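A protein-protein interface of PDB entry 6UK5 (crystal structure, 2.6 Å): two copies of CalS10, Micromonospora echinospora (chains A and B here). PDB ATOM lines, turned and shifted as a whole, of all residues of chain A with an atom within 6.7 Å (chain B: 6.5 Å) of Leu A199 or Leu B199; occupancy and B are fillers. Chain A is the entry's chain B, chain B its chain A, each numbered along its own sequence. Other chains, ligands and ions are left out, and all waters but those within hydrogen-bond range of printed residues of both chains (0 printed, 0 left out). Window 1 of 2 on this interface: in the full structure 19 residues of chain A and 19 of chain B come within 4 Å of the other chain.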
ATOM      1  N   LEU A 171      32.425  -7.895 -15.277  1.00  0.00           N
ATOM      2  CA  LEU A 171      32.889  -9.211 -15.709  1.00  0.00           C
ATOM      3  C   LEU A 171      34.281  -9.440 -15.135  1.00  0.00           C
ATOM      4  O   LEU A 171      35.239  -8.751 -15.504  1.00  0.00           O
ATOM      5  CB  LEU A 171      32.865  -9.322 -17.233  1.00  0.00           C
ATOM      6  CG  LEU A 171      33.342 -10.648 -17.818  1.00  0.00           C
ATOM      7  CD1 LEU A 171      32.347 -11.741 -17.516  1.00  0.00           C
ATOM      8  CD2 LEU A 171      33.485 -10.510 -19.329  1.00  0.00           C
ATOM      9  N   THR A 178      34.874 -17.787 -14.967  1.00  0.00           N
ATOM     10  CA  THR A 178      34.431 -16.476 -15.411  1.00  0.00           C
ATOM     11  C   THR A 178      33.158 -16.153 -14.644  1.00  0.00           C
ATOM     12  O   THR A 178      32.279 -17.009 -14.500  1.00  0.00           O
ATOM     13  CB  THR A 178      34.154 -16.428 -16.915  1.00  0.00           C
ATOM     14  OG1 THR A 178      35.238 -17.036 -17.627  1.00  0.00           O
ATOM     15  CG2 THR A 178      34.002 -14.982 -17.373  1.00  0.00           C
ATOM     16  N   VAL A 179      33.059 -14.924 -14.149  1.00  0.00           N
ATOM     17  CA  VAL A 179      31.946 -14.508 -13.308  1.00  0.00           C
ATOM     18  C   VAL A 179      31.307 -13.275 -13.920  1.00  0.00           C
ATOM     19  O   VAL A 179      31.984 -12.265 -14.144  1.00  0.00           O
ATOM     20  CB  VAL A 179      32.380 -14.227 -11.861  1.00  0.00           C
ATOM     21  CG1 VAL A 179      31.188 -13.756 -11.050  1.00  0.00           C
ATOM     22  CG2 VAL A 179      32.981 -15.474 -11.243  1.00  0.00           C
ATOM     23  N   ALA A 180      30.011 -13.360 -14.192  1.00  0.00           N
ATOM     24  CA  ALA A 180      29.226 -12.232 -14.660  1.00  0.00           C
ATOM     25  C   ALA A 180      28.337 -11.773 -13.518  1.00  0.00           C
ATOM     26  O   ALA A 180      27.857 -12.591 -12.728  1.00  0.00           O
ATOM     27  CB  ALA A 180      28.373 -12.609 -15.870  1.00  0.00           C
ATOM     28  N   ARG A 181      28.126 -10.464 -13.427  1.00  0.00           N
ATOM     29  CA  ARG A 181      27.299  -9.891 -12.376  1.00  0.00           C
ATOM     30  C   ARG A 181      26.522  -8.719 -12.944  1.00  0.00           C
ATOM     31  O   ARG A 181      27.103  -7.829 -13.571  1.00  0.00           O
ATOM     32  CB  ARG A 181      28.160  -9.438 -11.190  1.00  0.00           C
ATOM     33  CG  ARG A 181      27.382  -9.095  -9.927  1.00  0.00           C
ATOM     34  CD  ARG A 181      28.241  -8.251  -8.998  1.00  0.00           C
ATOM     35  NE  ARG A 181      28.512  -6.944  -9.592  1.00  0.00           N
ATOM     36  CZ  ARG A 181      27.923  -5.804  -9.241  1.00  0.00           C
ATOM     37  NH1 ARG A 181      27.023  -5.768  -8.268  1.00  0.00           N
ATOM     38  NH2 ARG A 181      28.251  -4.685  -9.869  1.00  0.00           N
ATOM     39  N   VAL A 182      25.210  -8.733 -12.735  1.00  0.00           N
ATOM     40  CA  VAL A 182      24.334  -7.611 -13.046  1.00  0.00           C
ATOM     41  C   VAL A 182      23.566  -7.255 -11.785  1.00  0.00           C
ATOM     42  O   VAL A 182      23.022  -8.140 -11.114  1.00  0.00           O
ATOM     43  CB  VAL A 182      23.374  -7.930 -14.205  1.00  0.00           C
ATOM     44  CG1 VAL A 182      22.400  -6.788 -14.407  1.00  0.00           C
ATOM     45  CG2 VAL A 182      24.164  -8.182 -15.482  1.00  0.00           C
ATOM     46  N   ARG A 197      22.805 -10.452  -9.155  1.00  0.00           N
ATOM     47  CA  ARG A 197      22.658 -11.758  -9.783  1.00  0.00           C
ATOM     48  C   ARG A 197      23.950 -12.110 -10.500  1.00  0.00           C
ATOM     49  O   ARG A 197      24.392 -11.371 -11.384  1.00  0.00           O
ATOM     50  CB  ARG A 197      21.468 -11.763 -10.745  1.00  0.00           C
ATOM     51  CG  ARG A 197      20.141 -11.722 -10.006  1.00  0.00           C
ATOM     52  CD  ARG A 197      18.956 -11.601 -10.935  1.00  0.00           C
ATOM     53  NE  ARG A 197      18.197 -12.839 -11.074  1.00  0.00           N
ATOM     54  CZ  ARG A 197      16.966 -12.898 -11.574  1.00  0.00           C
ATOM     55  NH1 ARG A 197      16.357 -11.791 -11.981  1.00  0.00           N
ATOM     56  NH2 ARG A 197      16.337 -14.060 -11.665  1.00  0.00           N
ATOM     57  N   TRP A 198      24.549 -13.232 -10.116  1.00  0.00           N
ATOM     58  CA  TRP A 198      25.827 -13.671 -10.647  1.00  0.00           C
ATOM     59  C   TRP A 198      25.628 -14.864 -11.573  1.00  0.00           C
ATOM     60  O   TRP A 198      24.684 -15.644 -11.423  1.00  0.00           O
ATOM     61  CB  TRP A 198      26.808 -14.073  -9.537  1.00  0.00           C
ATOM     62  CG  TRP A 198      27.277 -12.976  -8.633  1.00  0.00           C
ATOM     63  CD1 TRP A 198      28.388 -12.199  -8.805  1.00  0.00           C
ATOM     64  CD2 TRP A 198      26.681 -12.553  -7.401  1.00  0.00           C
ATOM     65  NE1 TRP A 198      28.512 -11.312  -7.763  1.00  0.00           N
ATOM     66  CE2 TRP A 198      27.477 -11.508  -6.888  1.00  0.00           C
ATOM     67  CE3 TRP A 198      25.548 -12.952  -6.686  1.00  0.00           C
ATOM     68  CZ2 TRP A 198      27.175 -10.856  -5.694  1.00  0.00           C
ATOM     69  CZ3 TRP A 198      25.249 -12.302  -5.500  1.00  0.00           C
ATOM     70  CH2 TRP A 198      26.059 -11.267  -5.017  1.00  0.00           C
ATOM     71  N   LEU A 199      26.537 -14.992 -12.534  1.00  0.00           N
ATOM     72  CA  LEU A 199      26.667 -16.192 -13.348  1.00  0.00           C
ATOM     73  C   LEU A 199      28.109 -16.656 -13.237  1.00  0.00           C
ATOM     74  O   LEU A 199      29.033 -15.899 -13.551  1.00  0.00           O
ATOM     75  CB  LEU A 199      26.283 -15.922 -14.804  1.00  0.00           C
ATOM     76  CG  LEU A 199      24.783 -15.779 -15.070  1.00  0.00           C
ATOM     77  CD1 LEU A 199      24.544 -15.378 -16.515  1.00  0.00           C
ATOM     78  CD2 LEU A 199      24.045 -17.065 -14.739  1.00  0.00           C
ATOM     79  N   VAL A 200      28.296 -17.898 -12.802  1.00  0.00           N
ATOM     80  CA  VAL A 200      29.614 -18.494 -12.636  1.00  0.00           C
ATOM     81  C   VAL A 200      29.722 -19.649 -13.624  1.00  0.00           C
ATOM     82  O   VAL A 200      28.983 -20.636 -13.516  1.00  0.00           O
ATOM     83  CB  VAL A 200      29.831 -18.989 -11.197  1.00  0.00           C
ATOM     84  CG1 VAL A 200      31.243 -19.531 -11.018  1.00  0.00           C
ATOM     85  CG2 VAL A 200      29.520 -17.891 -10.187  1.00  0.00           C
ATOM     86  N   GLY A 201      30.644 -19.530 -14.574  1.00  0.00           N
ATOM     87  CA  GLY A 201      30.918 -20.581 -15.538  1.00  0.00           C
ATOM     88  C   GLY A 201      32.326 -21.122 -15.349  1.00  0.00           C
ATOM     89  O   GLY A 201      33.285 -20.356 -15.238  1.00  0.00           O
ATOM     90  N   ILE A 206      27.694 -24.087 -15.472  1.00  0.00           N
ATOM     91  CA  ILE A 206      27.322 -22.700 -15.219  1.00  0.00           C
ATOM     92  C   ILE A 206      26.341 -22.681 -14.055  1.00  0.00           C
ATOM     93  O   ILE A 206      25.273 -23.303 -14.118  1.00  0.00           O
ATOM     94  CB  ILE A 206      26.715 -22.031 -16.458  1.00  0.00           C
ATOM     95  CG1 ILE A 206      27.675 -22.126 -17.643  1.00  0.00           C
ATOM     96  CG2 ILE A 206      26.444 -20.567 -16.163  1.00  0.00           C
ATOM     97  CD1 ILE A 206      27.076 -21.659 -18.954  1.00  0.00           C
ATOM     98  N   ARG A 207      26.708 -21.972 -12.996  1.00  0.00           N
ATOM     99  CA  ARG A 207      25.864 -21.769 -11.828  1.00  0.00           C
ATOM    100  C   ARG A 207      25.397 -20.324 -11.782  1.00  0.00           C
ATOM    101  O   ARG A 207      26.136 -19.409 -12.158  1.00  0.00           O
ATOM    102  CB  ARG A 207      26.628 -22.142 -10.560  1.00  0.00           C
ATOM    103  CG  ARG A 207      26.965 -23.618 -10.535  1.00  0.00           C
ATOM    104  CD  ARG A 207      27.692 -24.047  -9.279  1.00  0.00           C
ATOM    105  NE  ARG A 207      28.825 -23.173  -8.980  1.00  0.00           N
ATOM    106  CZ  ARG A 207      29.897 -23.032  -9.758  1.00  0.00           C
ATOM    107  NH1 ARG A 207      29.988 -23.677 -10.915  1.00  0.00           N
ATOM    108  NH2 ARG A 207      30.877 -22.221  -9.388  1.00  0.00           N
ATOM    109  N   GLU A 208      24.167 -20.126 -11.320  1.00  0.00           N
ATOM    110  CA  GLU A 208      23.605 -18.800 -11.125  1.00  0.00           C
ATOM    111  C   GLU A 208      23.373 -18.574  -9.638  1.00  0.00           C
ATOM    112  O   GLU A 208      22.999 -19.497  -8.908  1.00  0.00           O
ATOM    113  CB  GLU A 208      22.298 -18.635 -11.909  1.00  0.00           C
ATOM    114  CG  GLU A 208      21.239 -19.691 -11.623  1.00  0.00           C
ATOM    115  CD  GLU A 208      19.960 -19.445 -12.381  1.00  0.00           C
ATOM    116  OE1 GLU A 208      19.975 -18.616 -13.319  1.00  0.00           O
ATOM    117  OE2 GLU A 208      18.946 -20.088 -12.037  1.00  0.00           O
ATOM    118  N   PHE A 209      23.598 -17.339  -9.201  1.00  0.00           N
ATOM    119  CA  PHE A 209      23.378 -16.949  -7.821  1.00  0.00           C
ATOM    120  C   PHE A 209      22.699 -15.591  -7.794  1.00  0.00           C
ATOM    121  O   PHE A 209      22.923 -14.750  -8.669  1.00  0.00           O
ATOM    122  CB  PHE A 209      24.693 -16.845  -7.029  1.00  0.00           C
ATOM    123  CG  PHE A 209      25.489 -18.118  -6.978  1.00  0.00           C
ATOM    124  CD1 PHE A 209      26.348 -18.458  -8.011  1.00  0.00           C
ATOM    125  CD2 PHE A 209      25.398 -18.961  -5.883  1.00  0.00           C
ATOM    126  CE1 PHE A 209      27.087 -19.625  -7.960  1.00  0.00           C
ATOM    127  CE2 PHE A 209      26.134 -20.127  -5.826  1.00  0.00           C
ATOM    128  CZ  PHE A 209      26.981 -20.459  -6.867  1.00  0.00           C
ATOM    129  N   THR B 178      22.057  -3.275 -19.593  1.00  0.00           N
ATOM    130  CA  THR B 178      23.315  -4.009 -19.567  1.00  0.00           C
ATOM    131  C   THR B 178      23.035  -5.486 -19.794  1.00  0.00           C
ATOM    132  O   THR B 178      22.067  -6.034 -19.256  1.00  0.00           O
ATOM    133  CB  THR B 178      24.040  -3.823 -18.240  1.00  0.00           C
ATOM    134  OG1 THR B 178      23.818  -4.968 -17.410  1.00  0.00           O
ATOM    135  CG2 THR B 178      23.497  -2.612 -17.552  1.00  0.00           C
ATOM    136  N   VAL B 179      23.883  -6.125 -20.593  1.00  0.00           N
ATOM    137  CA  VAL B 179      23.689  -7.509 -20.999  1.00  0.00           C
ATOM    138  C   VAL B 179      24.938  -8.292 -20.623  1.00  0.00           C
ATOM    139  O   VAL B 179      26.037  -7.989 -21.100  1.00  0.00           O
ATOM    140  CB  VAL B 179      23.404  -7.608 -22.506  1.00  0.00           C
ATOM    141  CG1 VAL B 179      23.177  -9.049 -22.920  1.00  0.00           C
ATOM    142  CG2 VAL B 179      22.214  -6.722 -22.865  1.00  0.00           C
ATOM    143  N   ALA B 180      24.765  -9.291 -19.763  1.00  0.00           N
ATOM    144  CA  ALA B 180      25.821 -10.214 -19.379  1.00  0.00           C
ATOM    145  C   ALA B 180      25.525 -11.594 -19.946  1.00  0.00           C
ATOM    146  O   ALA B 180      24.364 -12.002 -20.057  1.00  0.00           O
ATOM    147  CB  ALA B 180      25.962 -10.300 -17.858  1.00  0.00           C
ATOM    148  N   ARG B 181      26.583 -12.311 -20.310  1.00  0.00           N
ATOM    149  CA  ARG B 181      26.433 -13.657 -20.841  1.00  0.00           C
ATOM    150  C   ARG B 181      27.588 -14.522 -20.368  1.00  0.00           C
ATOM    151  O   ARG B 181      28.748 -14.107 -20.446  1.00  0.00           O
ATOM    152  CB  ARG B 181      26.389 -13.678 -22.369  1.00  0.00           C
ATOM    153  CG  ARG B 181      25.867 -15.000 -22.915  1.00  0.00           C
ATOM    154  CD  ARG B 181      26.277 -15.220 -24.352  1.00  0.00           C
ATOM    155  NE  ARG B 181      27.713 -15.458 -24.457  1.00  0.00           N
ATOM    156  CZ  ARG B 181      28.369 -15.594 -25.604  1.00  0.00           C
ATOM    157  NH1 ARG B 181      27.721 -15.497 -26.757  1.00  0.00           N
ATOM    158  NH2 ARG B 181      29.677 -15.816 -25.594  1.00  0.00           N
ATOM    159  N   VAL B 182      27.266 -15.715 -19.882  1.00  0.00           N
ATOM    160  CA  VAL B 182      28.250 -16.748 -19.593  1.00  0.00           C
ATOM    161  C   VAL B 182      27.875 -17.954 -20.441  1.00  0.00           C
ATOM    162  O   VAL B 182      26.720 -18.395 -20.418  1.00  0.00           O
ATOM    163  CB  VAL B 182      28.276 -17.124 -18.101  1.00  0.00           C
ATOM    164  CG1 VAL B 182      29.272 -18.256 -17.854  1.00  0.00           C
ATOM    165  CG2 VAL B 182      28.593 -15.912 -17.246  1.00  0.00           C
ATOM    166  N   ARG B 197      23.812 -18.645 -20.853  1.00  0.00           N
ATOM    167  CA  ARG B 197      23.004 -18.092 -19.773  1.00  0.00           C
ATOM    168  C   ARG B 197      23.209 -16.588 -19.729  1.00  0.00           C
ATOM    169  O   ARG B 197      24.335 -16.113 -19.550  1.00  0.00           O
ATOM    170  CB  ARG B 197      23.351 -18.748 -18.439  1.00  0.00           C
ATOM    171  CG  ARG B 197      22.803 -20.158 -18.364  1.00  0.00           C
ATOM    172  CD  ARG B 197      23.188 -20.865 -17.092  1.00  0.00           C
ATOM    173  NE  ARG B 197      22.073 -20.851 -16.152  1.00  0.00           N
ATOM    174  CZ  ARG B 197      21.965 -21.650 -15.097  1.00  0.00           C
ATOM    175  NH1 ARG B 197      22.903 -22.554 -14.847  1.00  0.00           N
ATOM    176  NH2 ARG B 197      20.909 -21.551 -14.301  1.00  0.00           N
ATOM    177  N   TRP B 198      22.112 -15.852 -19.888  1.00  0.00           N
ATOM    178  CA  TRP B 198      22.127 -14.409 -20.046  1.00  0.00           C
ATOM    179  C   TRP B 198      21.560 -13.712 -18.817  1.00  0.00           C
ATOM    180  O   TRP B 198      20.710 -14.256 -18.107  1.00  0.00           O
ATOM    181  CB  TRP B 198      21.298 -14.004 -21.269  1.00  0.00           C
ATOM    182  CG  TRP B 198      21.782 -14.581 -22.561  1.00  0.00           C
ATOM    183  CD1 TRP B 198      21.621 -15.866 -22.992  1.00  0.00           C
ATOM    184  CD2 TRP B 198      22.487 -13.895 -23.601  1.00  0.00           C
ATOM    185  NE1 TRP B 198      22.186 -16.023 -24.234  1.00  0.00           N
ATOM    186  CE2 TRP B 198      22.726 -14.827 -24.629  1.00  0.00           C
ATOM    187  CE3 TRP B 198      22.943 -12.584 -23.760  1.00  0.00           C
ATOM    188  CZ2 TRP B 198      23.402 -14.492 -25.800  1.00  0.00           C
ATOM    189  CZ3 TRP B 198      23.615 -12.252 -24.924  1.00  0.00           C
ATOM    190  CH2 TRP B 198      23.837 -13.202 -25.928  1.00  0.00           C
ATOM    191  N   LEU B 199      22.050 -12.499 -18.573  1.00  0.00           N
ATOM    192  CA  LEU B 199      21.449 -11.576 -17.618  1.00  0.00           C
ATOM    193  C   LEU B 199      21.240 -10.237 -18.307  1.00  0.00           C
ATOM    194  O   LEU B 199      22.199  -9.648 -18.816  1.00  0.00           O
ATOM    195  CB  LEU B 199      22.327 -11.393 -16.378  1.00  0.00           C
ATOM    196  CG  LEU B 199      22.370 -12.514 -15.342  1.00  0.00           C
ATOM    197  CD1 LEU B 199      23.410 -12.180 -14.283  1.00  0.00           C
ATOM    198  CD2 LEU B 199      21.010 -12.722 -14.698  1.00  0.00           C
ATOM    199  N   VAL B 200      19.998  -9.764 -18.337  1.00  0.00           N
ATOM    200  CA  VAL B 200      19.671  -8.450 -18.879  1.00  0.00           C
ATOM    201  C   VAL B 200      19.060  -7.609 -17.768  1.00  0.00           C
ATOM    202  O   VAL B 200      18.002  -7.957 -17.225  1.00  0.00           O
ATOM    203  CB  VAL B 200      18.728  -8.531 -20.088  1.00  0.00           C
ATOM    204  CG1 VAL B 200      18.418  -7.131 -20.596  1.00  0.00           C
ATOM    205  CG2 VAL B 200      19.370  -9.348 -21.193  1.00  0.00           C
ATOM    206  N   GLY B 201      19.728  -6.510 -17.430  1.00  0.00           N
ATOM    207  CA  GLY B 201      19.216  -5.535 -16.483  1.00  0.00           C
ATOM    208  C   GLY B 201      18.936  -4.232 -17.212  1.00  0.00           C
ATOM    209  O   GLY B 201      19.767  -3.752 -17.984  1.00  0.00           O
ATOM    210  N   ILE B 206      15.825  -6.945 -13.678  1.00  0.00           N
ATOM    211  CA  ILE B 206      16.854  -7.906 -14.061  1.00  0.00           C
ATOM    212  C   ILE B 206      16.162  -9.162 -14.574  1.00  0.00           C
ATOM    213  O   ILE B 206      15.406  -9.804 -13.834  1.00  0.00           O
ATOM    214  CB  ILE B 206      17.777  -8.250 -12.880  1.00  0.00           C
ATOM    215  CG1 ILE B 206      18.465  -7.005 -12.317  1.00  0.00           C
ATOM    216  CG2 ILE B 206      18.804  -9.288 -13.309  1.00  0.00           C
ATOM    217  CD1 ILE B 206      19.229  -7.261 -11.020  1.00  0.00           C
ATOM    218  N   ARG B 207      16.416  -9.523 -15.831  1.00  0.00           N
ATOM    219  CA  ARG B 207      15.905 -10.762 -16.398  1.00  0.00           C
ATOM    220  C   ARG B 207      17.041 -11.751 -16.638  1.00  0.00           C
ATOM    221  O   ARG B 207      18.135 -11.362 -17.062  1.00  0.00           O
ATOM    222  CB  ARG B 207      15.181 -10.530 -17.731  1.00  0.00           C
ATOM    223  CG  ARG B 207      13.972  -9.614 -17.666  1.00  0.00           C
ATOM    224  CD  ARG B 207      13.171  -9.659 -18.969  1.00  0.00           C
ATOM    225  NE  ARG B 207      13.969  -9.538 -20.189  1.00  0.00           N
ATOM    226  CZ  ARG B 207      14.624  -8.446 -20.570  1.00  0.00           C
ATOM    227  NH1 ARG B 207      14.603  -7.351 -19.823  1.00  0.00           N
ATOM    228  NH2 ARG B 207      15.309  -8.453 -21.708  1.00  0.00           N
ATOM    229  N   GLU B 208      16.777 -13.029 -16.364  1.00  0.00           N
ATOM    230  CA  GLU B 208      17.673 -14.123 -16.720  1.00  0.00           C
ATOM    231  C   GLU B 208      16.959 -15.115 -17.629  1.00  0.00           C
ATOM    232  O   GLU B 208      15.773 -15.401 -17.436  1.00  0.00           O
ATOM    233  CB  GLU B 208      18.182 -14.860 -15.478  1.00  0.00           C
ATOM    234  CG  GLU B 208      17.076 -15.299 -14.536  1.00  0.00           C
ATOM    235  CD  GLU B 208      17.583 -16.154 -13.401  1.00  0.00           C
ATOM    236  OE1 GLU B 208      16.736 -16.765 -12.712  1.00  0.00           O
ATOM    237  OE2 GLU B 208      18.818 -16.214 -13.205  1.00  0.00           O
ATOM    238  N   PHE B 209      17.675 -15.635 -18.625  1.00  0.00           N
ATOM    239  CA  PHE B 209      17.159 -16.725 -19.447  1.00  0.00           C
ATOM    240  C   PHE B 209      18.325 -17.634 -19.822  1.00  0.00           C
ATOM    241  O   PHE B 209      19.473 -17.188 -19.911  1.00  0.00           O
ATOM    242  CB  PHE B 209      16.384 -16.218 -20.676  1.00  0.00           C
ATOM    243  CG  PHE B 209      17.224 -15.545 -21.720  1.00  0.00           C
ATOM    244  CD1 PHE B 209      17.473 -14.184 -21.660  1.00  0.00           C
ATOM    245  CD2 PHE B 209      17.729 -16.268 -22.789  1.00  0.00           C
ATOM    246  CE1 PHE B 209      18.232 -13.561 -22.632  1.00  0.00           C
ATOM    247  CE2 PHE B 209      18.486 -15.653 -23.763  1.00  0.00           C
ATOM    248  CZ  PHE B 209      18.738 -14.296 -23.687  1.00  0.00           C
ATOM    249  N   SER B 210      18.019 -18.919 -20.031  1.00  0.00           N
ATOM    250  CA  SER B 210      19.024 -19.948 -20.272  1.00  0.00           C
ATOM    251  C   SER B 210      18.636 -20.804 -21.470  1.00  0.00           C
ATOM    252  O   SER B 210      17.454 -21.082 -21.694  1.00  0.00           O
ATOM    253  CB  SER B 210      19.205 -20.843 -19.037  1.00  0.00           C
ATOM    254  OG  SER B 210      19.257 -20.061 -17.856  1.00  0.00           O
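The backbone carbonyl oxygen of Ile A206 lies within hydrogen-bond range of the guanidinium group of Arg B197, 2.6 Å away. NH2 of Arg B197 is in salt-bridge range of OE1 of Glu A208 (3.2 Å). The backbone carbonyl oxygen (O) of Ile B206 is in hydrogen-bond range of the guanidinium group (NH1) of Arg A197, at 2.9 Å. OE1 of Glu B208 is in salt-bridge range of NH2 of Arg A197. The side-chain carboxylate (OE2) of Glu B208 sits close to the side-chain carboxylate (OE1) of Glu A208, at 2.7 Å.
N of Thr B178 sits at hydrogen-bond distance from O of Gly B201, at 2.8 Å. The backbone carbonyl oxygen (O) of Leu B199 is in hydrogen-bond range of the backbone NH (N) of Ala B180 (2.8 Å). N of Arg B197 sits at hydrogen-bond distance from O of Val B182 (3.0 Å). The backbone carbonyl oxygen of Thr A178 sits at hydrogen-bond distance from the backbone NH of Gly A201, 3.0 Å away. The backbone carbonyl oxygen (O) of Ala A180 is in hydrogen-bond range of the backbone NH (N) of Leu A199. The backbone carbonyl oxygen (O) of Val A182 is in hydrogen-bond range of the backbone NH (N) of Arg A197, at 3.0 Å.
CB of Ala B180 touches CB of Ala A180, 3.9 Å away. CG2 of Val A182 touches OG1 of Thr B178, 3.8 Å away. Val A182 touches Ala B180 (CG2 to CB, 3.7 Å). Val A182 touches Leu B199 (CG2 to CB, 3.8 Å). Val A182 touches Ile B206. Val B182 touches Leu A199 (CG2 to CB, 3.4 Å). Leu A199 touches Arg B197 (CD1 to O, 3.1 Å). CG of Leu B199 touches CD1 of Leu A199, 3.8 Å away. CG1 of Val B182 touches CA of Gly A201 (3.7 Å). CD1 of Ile A206 touches O of Val B182 (3.6 Å).
Of chain B, only Val B182 (3.4 Å), Arg B197 (3.1 Å) and Leu B199 (3.8 Å) come within 4 Å of Leu A199. Leu B199 touches three residues of chain A. Of the printed residues of chain A, Val B182 touches Ala A180 (3.6 Å), Leu A199 (3.4 Å), Gly A201 (3.7 Å) and Ile A206 (3.6 Å). Printed residues of chain A within 4 Å of Thr B178: Val A182. The nearest residue of chain B that does not touch Leu A199 is Trp B198 (4.1 Å). The nearest residue of chain A that does not touch Leu B199 is Trp A198 (4.4 Å).
Printed residues of chain A that touch a printed residue of chain B: Ala A180, Val A182, Arg A197, Leu A199, Gly A201, Ile A206 and Glu A208. Along chain A the printed residues that touch a printed residue of chain B span positions 180 to 208. Hydrophobic or aromatic side chains of chain B that line the printed part of chain A: Ala B180, Val B182, Leu B199 and Ile B206. Among the printed residues, 17 pairs touch across the chains. Among the printed residues, Asp or Glu carboxylates within 4 Å of a Lys or Arg side-chain nitrogen of the other chain: Arg A197 with Glu B208 and Glu A208 with Arg B197.
Val A182 touches Leu B199, and with the chains exchanged Leu A199 touches Val B182. Val A182 touches Ile B206, and with the chains exchanged Ile A206 touches Val B182. Arg A197 touches Glu B208, and with the chains exchanged Glu A208 touches Arg B197. Glu A208 touches its own counterpart, Glu B208. Of the 17 pairs that touch across the chains among the printed residues, 15 have their exchanged pair printed and touching as well.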
